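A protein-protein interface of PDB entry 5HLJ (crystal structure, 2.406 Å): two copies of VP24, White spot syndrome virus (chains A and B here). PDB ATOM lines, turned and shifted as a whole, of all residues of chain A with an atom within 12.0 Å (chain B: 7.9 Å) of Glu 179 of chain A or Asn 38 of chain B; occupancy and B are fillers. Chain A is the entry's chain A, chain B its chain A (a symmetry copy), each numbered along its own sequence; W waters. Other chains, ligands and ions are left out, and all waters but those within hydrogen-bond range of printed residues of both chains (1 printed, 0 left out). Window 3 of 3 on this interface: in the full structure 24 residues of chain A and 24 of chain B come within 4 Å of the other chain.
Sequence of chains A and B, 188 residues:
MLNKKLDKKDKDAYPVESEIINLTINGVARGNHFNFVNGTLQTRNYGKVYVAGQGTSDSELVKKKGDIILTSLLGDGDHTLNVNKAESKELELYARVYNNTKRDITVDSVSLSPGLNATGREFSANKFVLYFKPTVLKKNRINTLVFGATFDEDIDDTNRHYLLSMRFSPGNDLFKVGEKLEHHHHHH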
ATOM      1  N   LEU A 174       2.668 -13.963  -4.594  1.00  0.00           N
ATOM      2  CA  LEU A 174       1.374 -13.987  -3.916  1.00  0.00           C
ATOM      3  C   LEU A 174       0.465 -12.898  -4.478  1.00  0.00           C
ATOM      4  O   LEU A 174       0.930 -11.934  -5.106  1.00  0.00           O
ATOM      5  CB  LEU A 174       1.542 -13.785  -2.413  1.00  0.00           C
ATOM      6  CG  LEU A 174       2.313 -14.837  -1.613  1.00  0.00           C
ATOM      7  CD1 LEU A 174       2.549 -14.323  -0.200  1.00  0.00           C
ATOM      8  CD2 LEU A 174       1.567 -16.169  -1.585  1.00  0.00           C
ATOM      9  N   PHE A 175      -0.831 -13.058  -4.247  1.00  0.00           N
ATOM     10  CA  PHE A 175      -1.810 -12.082  -4.686  1.00  0.00           C
ATOM     11  C   PHE A 175      -1.485 -10.674  -4.180  1.00  0.00           C
ATOM     12  O   PHE A 175      -1.268 -10.468  -2.986  1.00  0.00           O
ATOM     13  CB  PHE A 175      -3.204 -12.498  -4.219  1.00  0.00           C
ATOM     14  CG  PHE A 175      -4.299 -11.608  -4.729  1.00  0.00           C
ATOM     15  CD1 PHE A 175      -4.580 -11.540  -6.093  1.00  0.00           C
ATOM     16  CD2 PHE A 175      -5.052 -10.841  -3.850  1.00  0.00           C
ATOM     17  CE1 PHE A 175      -5.589 -10.719  -6.574  1.00  0.00           C
ATOM     18  CE2 PHE A 175      -6.068 -10.017  -4.321  1.00  0.00           C
ATOM     19  CZ  PHE A 175      -6.341  -9.965  -5.688  1.00  0.00           C
ATOM     20  N   LYS A 176      -1.441  -9.709  -5.090  1.00  0.00           N
ATOM     21  CA  LYS A 176      -1.251  -8.317  -4.690  1.00  0.00           C
ATOM     22  C   LYS A 176      -2.568  -7.517  -4.816  1.00  0.00           C
ATOM     23  O   LYS A 176      -3.046  -7.226  -5.919  1.00  0.00           O
ATOM     24  CB  LYS A 176      -0.120  -7.676  -5.512  1.00  0.00           C
ATOM     25  CG  LYS A 176      -0.103  -6.148  -5.430  1.00  0.00           C
ATOM     26  CD  LYS A 176       1.238  -5.525  -5.831  1.00  0.00           C
ATOM     27  CE  LYS A 176       1.203  -3.997  -5.669  1.00  0.00           C
ATOM     28  NZ  LYS A 176       1.815  -3.558  -4.365  1.00  0.00           N
ATOM     29  N   VAL A 177      -3.156  -7.187  -3.672  1.00  0.00           N
ATOM     30  CA  VAL A 177      -4.402  -6.431  -3.628  1.00  0.00           C
ATOM     31  C   VAL A 177      -4.318  -5.075  -4.336  1.00  0.00           C
ATOM     32  O   VAL A 177      -3.405  -4.296  -4.088  1.00  0.00           O
ATOM     33  CB  VAL A 177      -4.840  -6.199  -2.177  1.00  0.00           C
ATOM     34  CG1 VAL A 177      -6.053  -5.299  -2.132  1.00  0.00           C
ATOM     35  CG2 VAL A 177      -5.149  -7.525  -1.516  1.00  0.00           C
ATOM     36  N   GLY A 178      -5.279  -4.799  -5.215  1.00  0.00           N
ATOM     37  CA  GLY A 178      -5.338  -3.538  -5.939  1.00  0.00           C
ATOM     38  C   GLY A 178      -6.013  -2.405  -5.176  1.00  0.00           C
ATOM     39  O   GLY A 178      -6.252  -2.504  -3.974  1.00  0.00           O
ATOM     40  N   GLU A 179      -6.325  -1.326  -5.887  1.00  0.00           N
ATOM     41  CA  GLU A 179      -6.899  -0.133  -5.266  1.00  0.00           C
ATOM     42  C   GLU A 179      -8.405  -0.253  -5.048  1.00  0.00           C
ATOM     43  O   GLU A 179      -9.090  -0.942  -5.800  1.00  0.00           O
ATOM     44  CB  GLU A 179      -6.598   1.099  -6.118  1.00  0.00           C
ATOM     45  CG  GLU A 179      -5.111   1.368  -6.315  1.00  0.00           C
ATOM     46  CD  GLU A 179      -4.423   1.852  -5.046  1.00  0.00           C
ATOM     47  OE1 GLU A 179      -5.131   2.265  -4.096  1.00  0.00           O
ATOM     48  OE2 GLU A 179      -3.172   1.824  -5.005  1.00  0.00           O
ATOM     49  N   LYS A 180      -8.907   0.434  -4.021  1.00  0.00           N
ATOM     50  CA  LYS A 180     -10.324   0.382  -3.645  1.00  0.00           C
ATOM     51  C   LYS A 180     -11.270   0.929  -4.724  1.00  0.00           C
ATOM     52  O   LYS A 180     -10.869   1.689  -5.606  1.00  0.00           O
ATOM     53  CB  LYS A 180     -10.548   1.148  -2.334  1.00  0.00           C
ATOM     54  CG  LYS A 180     -10.002   0.453  -1.092  1.00  0.00           C
ATOM     55  CD  LYS A 180      -8.856   1.238  -0.464  1.00  0.00           C
ATOM     56  CE  LYS A 180      -8.435   0.633   0.870  1.00  0.00           C
ATOM     57  NZ  LYS A 180      -7.201   1.269   1.420  1.00  0.00           N
ATOM     58  N   LEU B  23      -6.520 -16.690  -4.289  1.00  0.00           N
ATOM     59  CA  LEU B  23      -7.200 -15.403  -4.345  1.00  0.00           C
ATOM     60  C   LEU B  23      -8.005 -15.143  -3.074  1.00  0.00           C
ATOM     61  O   LEU B  23      -8.298 -16.060  -2.303  1.00  0.00           O
ATOM     62  CB  LEU B  23      -8.141 -15.343  -5.548  1.00  0.00           C
ATOM     63  CG  LEU B  23      -7.535 -15.527  -6.937  1.00  0.00           C
ATOM     64  CD1 LEU B  23      -8.630 -15.412  -7.966  1.00  0.00           C
ATOM     65  CD2 LEU B  23      -6.437 -14.490  -7.190  1.00  0.00           C
ATOM     66  N   THR B  24      -8.393 -13.890  -2.880  1.00  0.00           N
ATOM     67  CA  THR B  24      -9.210 -13.513  -1.740  1.00  0.00           C
ATOM     68  C   THR B  24     -10.643 -13.218  -2.176  1.00  0.00           C
ATOM     69  O   THR B  24     -10.855 -12.628  -3.227  1.00  0.00           O
ATOM     70  CB  THR B  24      -8.588 -12.300  -1.021  1.00  0.00           C
ATOM     71  OG1 THR B  24      -7.310 -12.684  -0.505  1.00  0.00           O
ATOM     72  CG2 THR B  24      -9.439 -11.864   0.129  1.00  0.00           C
ATOM     73  N   ASN B  26     -14.911 -12.300  -0.623  1.00  0.00           N
ATOM     74  CA  ASN B  26     -15.838 -12.003   0.465  1.00  0.00           C
ATOM     75  C   ASN B  26     -17.267 -12.431   0.141  1.00  0.00           C
ATOM     76  O   ASN B  26     -17.717 -12.307  -0.991  1.00  0.00           O
ATOM     77  CB  ASN B  26     -15.823 -10.506   0.797  1.00  0.00           C
ATOM     78  CG  ASN B  26     -14.497 -10.048   1.370  1.00  0.00           C
ATOM     79  OD1 ASN B  26     -14.110 -10.452   2.461  1.00  0.00           O
ATOM     80  ND2 ASN B  26     -13.799  -9.192   0.637  1.00  0.00           N
ATOM     81  N   ASN B  35     -17.679 -12.498  -3.713  1.00  0.00           N
ATOM     82  CA  ASN B  35     -17.168 -11.376  -4.486  1.00  0.00           C
ATOM     83  C   ASN B  35     -15.641 -11.301  -4.398  1.00  0.00           C
ATOM     84  O   ASN B  35     -15.075 -11.330  -3.297  1.00  0.00           O
ATOM     85  CB  ASN B  35     -17.812 -10.076  -3.984  1.00  0.00           C
ATOM     86  CG  ASN B  35     -17.619  -8.918  -4.940  1.00  0.00           C
ATOM     87  OD1 ASN B  35     -17.533  -9.103  -6.156  1.00  0.00           O
ATOM     88  ND2 ASN B  35     -17.555  -7.711  -4.393  1.00  0.00           N
ATOM     89  N   PHE B  36     -14.970 -11.232  -5.550  1.00  0.00           N
ATOM     90  CA  PHE B  36     -13.507 -11.140  -5.558  1.00  0.00           C
ATOM     91  C   PHE B  36     -13.012  -9.867  -4.878  1.00  0.00           C
ATOM     92  O   PHE B  36     -13.713  -8.861  -4.853  1.00  0.00           O
ATOM     93  CB  PHE B  36     -12.953 -11.172  -6.977  1.00  0.00           C
ATOM     94  CG  PHE B  36     -13.040 -12.516  -7.644  1.00  0.00           C
ATOM     95  CD1 PHE B  36     -12.441 -13.641  -7.064  1.00  0.00           C
ATOM     96  CD2 PHE B  36     -13.681 -12.654  -8.875  1.00  0.00           C
ATOM     97  CE1 PHE B  36     -12.507 -14.883  -7.691  1.00  0.00           C
ATOM     98  CE2 PHE B  36     -13.757 -13.890  -9.506  1.00  0.00           C
ATOM     99  CZ  PHE B  36     -13.160 -15.010  -8.907  1.00  0.00           C
ATOM    100  N   VAL B  37     -11.804  -9.923  -4.325  1.00  0.00           N
ATOM    101  CA  VAL B  37     -11.028  -8.723  -4.045  1.00  0.00           C
ATOM    102  C   VAL B  37     -10.194  -8.454  -5.290  1.00  0.00           C
ATOM    103  O   VAL B  37      -9.520  -9.355  -5.797  1.00  0.00           O
ATOM    104  CB  VAL B  37     -10.120  -8.890  -2.809  1.00  0.00           C
ATOM    105  CG1 VAL B  37      -9.149  -7.720  -2.695  1.00  0.00           C
ATOM    106  CG2 VAL B  37     -10.959  -9.041  -1.547  1.00  0.00           C
ATOM    107  N   ASN B  38     -10.251  -7.242  -5.822  1.00  0.00           N
ATOM    108  CA  ASN B  38      -9.529  -6.958  -7.068  1.00  0.00           C
ATOM    109  C   ASN B  38      -8.033  -6.868  -6.802  1.00  0.00           C
ATOM    110  O   ASN B  38      -7.616  -6.585  -5.674  1.00  0.00           O
ATOM    111  CB  ASN B  38     -10.043  -5.673  -7.719  1.00  0.00           C
ATOM    112  CG  ASN B  38      -9.887  -4.470  -6.823  1.00  0.00           C
ATOM    113  OD1 ASN B  38     -10.621  -4.313  -5.844  1.00  0.00           O
ATOM    114  ND2 ASN B  38      -8.932  -3.604  -7.153  1.00  0.00           N
ATOM    115  N   GLY B  39      -7.232  -7.129  -7.831  1.00  0.00           N
ATOM    116  CA  GLY B  39      -5.790  -7.163  -7.677  1.00  0.00           C
ATOM    117  C   GLY B  39      -5.199  -8.034  -8.760  1.00  0.00           C
ATOM    118  O   GLY B  39      -5.885  -8.372  -9.728  1.00  0.00           O
ATOM    119  N   THR B  40      -3.930  -8.406  -8.596  1.00  0.00           N
ATOM    120  CA  THR B  40      -3.207  -9.162  -9.613  1.00  0.00           C
ATOM    121  C   THR B  40      -2.369 -10.249  -8.975  1.00  0.00           C
ATOM    122  O   THR B  40      -2.063 -10.209  -7.778  1.00  0.00           O
ATOM    123  CB  THR B  40      -2.279  -8.259 -10.473  1.00  0.00           C
ATOM    124  OG1 THR B  40      -1.390  -7.543  -9.616  1.00  0.00           O
ATOM    125  CG2 THR B  40      -3.082  -7.254 -11.289  1.00  0.00           C
ATOM    126  N   TYR B  50      -5.363 -11.349 -13.631  1.00  0.00           N
ATOM    127  CA  TYR B  50      -5.912 -10.025 -13.357  1.00  0.00           C
ATOM    128  C   TYR B  50      -7.333 -10.164 -12.851  1.00  0.00           C
ATOM    129  O   TYR B  50      -8.227 -10.633 -13.571  1.00  0.00           O
ATOM    130  CB  TYR B  50      -5.875  -9.140 -14.620  1.00  0.00           C
ATOM    131  CG  TYR B  50      -6.264  -7.677 -14.427  1.00  0.00           C
ATOM    132  CD1 TYR B  50      -5.323  -6.659 -14.604  1.00  0.00           C
ATOM    133  CD2 TYR B  50      -7.570  -7.306 -14.120  1.00  0.00           C
ATOM    134  CE1 TYR B  50      -5.665  -5.322 -14.457  1.00  0.00           C
ATOM    135  CE2 TYR B  50      -7.921  -5.970 -13.967  1.00  0.00           C
ATOM    136  CZ  TYR B  50      -6.958  -4.984 -14.140  1.00  0.00           C
ATOM    137  OH  TYR B  50      -7.302  -3.665 -13.995  1.00  0.00           O
ATOM    138  N   VAL B  51      -7.553  -9.723 -11.625  1.00  0.00           N
ATOM    139  CA  VAL B  51      -8.880  -9.772 -11.065  1.00  0.00           C
ATOM    140  C   VAL B  51      -9.509  -8.383 -11.123  1.00  0.00           C
ATOM    141  O   VAL B  51      -9.227  -7.543 -10.269  1.00  0.00           O
ATOM    142  CB  VAL B  51      -8.851 -10.289  -9.612  1.00  0.00           C
ATOM    143  CG1 VAL B  51     -10.250 -10.381  -9.046  1.00  0.00           C
ATOM    144  CG2 VAL B  51      -8.155 -11.646  -9.545  1.00  0.00           C
ATOM    145  N   ALA B  52     -10.366  -8.152 -12.123  1.00  0.00           N
ATOM    146  CA  ALA B  52     -11.027  -6.852 -12.304  1.00  0.00           C
ATOM    147  C   ALA B  52     -12.044  -6.554 -11.213  1.00  0.00           C
ATOM    148  O   ALA B  52     -12.364  -7.414 -10.390  1.00  0.00           O
ATOM    149  CB  ALA B  52     -11.701  -6.786 -13.675  1.00  0.00           C
ATOM    150  N   GLY B  53     -12.558  -5.330 -11.202  1.00  0.00           N
ATOM    151  CA  GLY B  53     -13.617  -4.975 -10.270  1.00  0.00           C
ATOM    152  C   GLY B  53     -14.914  -5.738 -10.528  1.00  0.00           C
ATOM    153  O   GLY B  53     -15.142  -6.263 -11.620  1.00  0.00           O
ATOM    154  N   GLN B  54     -15.776  -5.783  -9.524  1.00  0.00           N
ATOM    155  CA  GLN B  54     -17.041  -6.493  -9.644  1.00  0.00           C
ATOM    156  C   GLN B  54     -17.887  -6.021 -10.820  1.00  0.00           C
ATOM    157  O   GLN B  54     -17.894  -4.846 -11.169  1.00  0.00           O
ATOM    158  CB  GLN B  54     -17.836  -6.349  -8.358  1.00  0.00           C
ATOM    159  CG  GLN B  54     -18.135  -4.912  -8.001  1.00  0.00           C
ATOM    160  CD  GLN B  54     -18.565  -4.758  -6.548  1.00  0.00           C
ATOM    161  OE1 GLN B  54     -17.834  -5.138  -5.625  1.00  0.00           O
ATOM    162  NE2 GLN B  54     -19.753  -4.200  -6.339  1.00  0.00           N
ATOM    163  N   LEU B  70     -10.497 -12.115 -14.581  1.00  0.00           N
ATOM    164  CA  LEU B  70     -11.659 -12.586 -13.860  1.00  0.00           C
ATOM    165  C   LEU B  70     -12.486 -11.433 -13.321  1.00  0.00           C
ATOM    166  O   LEU B  70     -11.939 -10.403 -12.922  1.00  0.00           O
ATOM    167  CB  LEU B  70     -11.253 -13.486 -12.695  1.00  0.00           C
ATOM    168  CG  LEU B  70     -10.390 -14.723 -12.929  1.00  0.00           C
ATOM    169  CD1 LEU B  70      -8.910 -14.377 -12.904  1.00  0.00           C
ATOM    170  CD2 LEU B  70     -10.721 -15.737 -11.862  1.00  0.00           C
ATOM    171  N   SER B  72     -16.203 -11.203 -10.703  1.00  0.00           N
ATOM    172  CA  SER B  72     -17.364 -11.804 -10.072  1.00  0.00           C
ATOM    173  C   SER B  72     -18.571 -10.902 -10.305  1.00  0.00           C
ATOM    174  O   SER B  72     -18.457  -9.677 -10.219  1.00  0.00           O
ATOM    175  CB  SER B  72     -17.124 -12.030  -8.581  1.00  0.00           C
ATOM    176  OG  SER B  72     -16.684 -10.848  -7.941  1.00  0.00           O
HETATM  177  O   HOH W   1      -2.142  -5.702  -8.169  1.00  0.00           O
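The backbone carbonyl oxygen (O) of Thr 40 of chain B is in hydrogen-bond range of the backbone NH (N) of Lys 176 of chain A, at 2.8 Å.
The backbone NH of Gly 178 of chain A lies within hydrogen-bond range of the backbone carbonyl oxygen of Asn 38 of chain B, 3.0 Å away.
The side-chain amide nitrogen (ND2) of Asn 38 of chain B is in hydrogen-bond range of the backbone carbonyl oxygen (O) of Glu 179 of chain A (3.0 Å).
The backbone carbonyl oxygen of Thr 24 of chain B sits at hydrogen-bond distance from the backbone NH of Val 37 of chain B, at 3.1 Å.
O of Gly 39 of chain B is in hydrogen-bond range of N of Val 51 of chain B.
Leu 23 of chain B touches Phe 175 of chain A.
Val 37 of chain B touches Phe 175 of chain A (O to CZ, 3.2 Å).
Asn 38 of chain B touches Phe 175 of chain A (O to CZ, 3.6 Å).
Phe 175 of chain A touches Gly 39 of chain B (CZ to CA, 3.5 Å).
Phe 175 of chain A touches Thr 40 of chain B (CD1 to O, 3.3 Å).
O of Lys 176 of chain A touches CA of Gly 39 of chain B (3.3 Å).
CG1 of Val 37 of chain B touches CG1 of Val 177 of chain A, 3.97 Å away.
Asn 38 of chain B touches Val 177 of chain A.
Gly 178 of chain A touches Gly 39 of chain B.
Of the printed residues of chain B, Phe 175 of chain A touches Leu 23 (3.7 Å), Val 37 (3.2 Å), Asn 38 (3.6 Å), Gly 39 (3.5 Å) and Thr 40 (3.3 Å).
Glu 179 of chain A touches one residue of chain B.
Of the printed residues of chain A, Leu 23 of chain B touches Phe 175 (3.7 Å).
Thr 24 of chain B touches none of the printed residues of chain A.
Printed residues of chain A within 4 Å of Asn 38 of chain B: Phe 175 (3.6 Å), Val 177 (3.8 Å), Gly 178 (3.0 Å) and Glu 179 (3.0 Å).
Thr 40 of chain B touches just these residues of chain A: Phe 175 (3.3 Å) and Lys 176 (2.8 Å).
No residue of chain A comes within 4 Å of Val 51 of chain B.
The nearest printed residue of chain A that does not touch Leu 23 of chain B is Lys 176 of chain A (7.2 Å).
Of the 16 printed residues of chain B, 5 touch a printed residue of chain A.
Among the printed residues, 12 pairs touch across the chains.
No position is printed for both chains.
Of the 12 pairs that touch across the chains among the printed residues, none has its exchanged pair printed and touching as well.
Water W1 bridges OG1 of Thr 40 of chain B (2.5 Å) and O of Lys 176 of chain A (2.9 Å).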
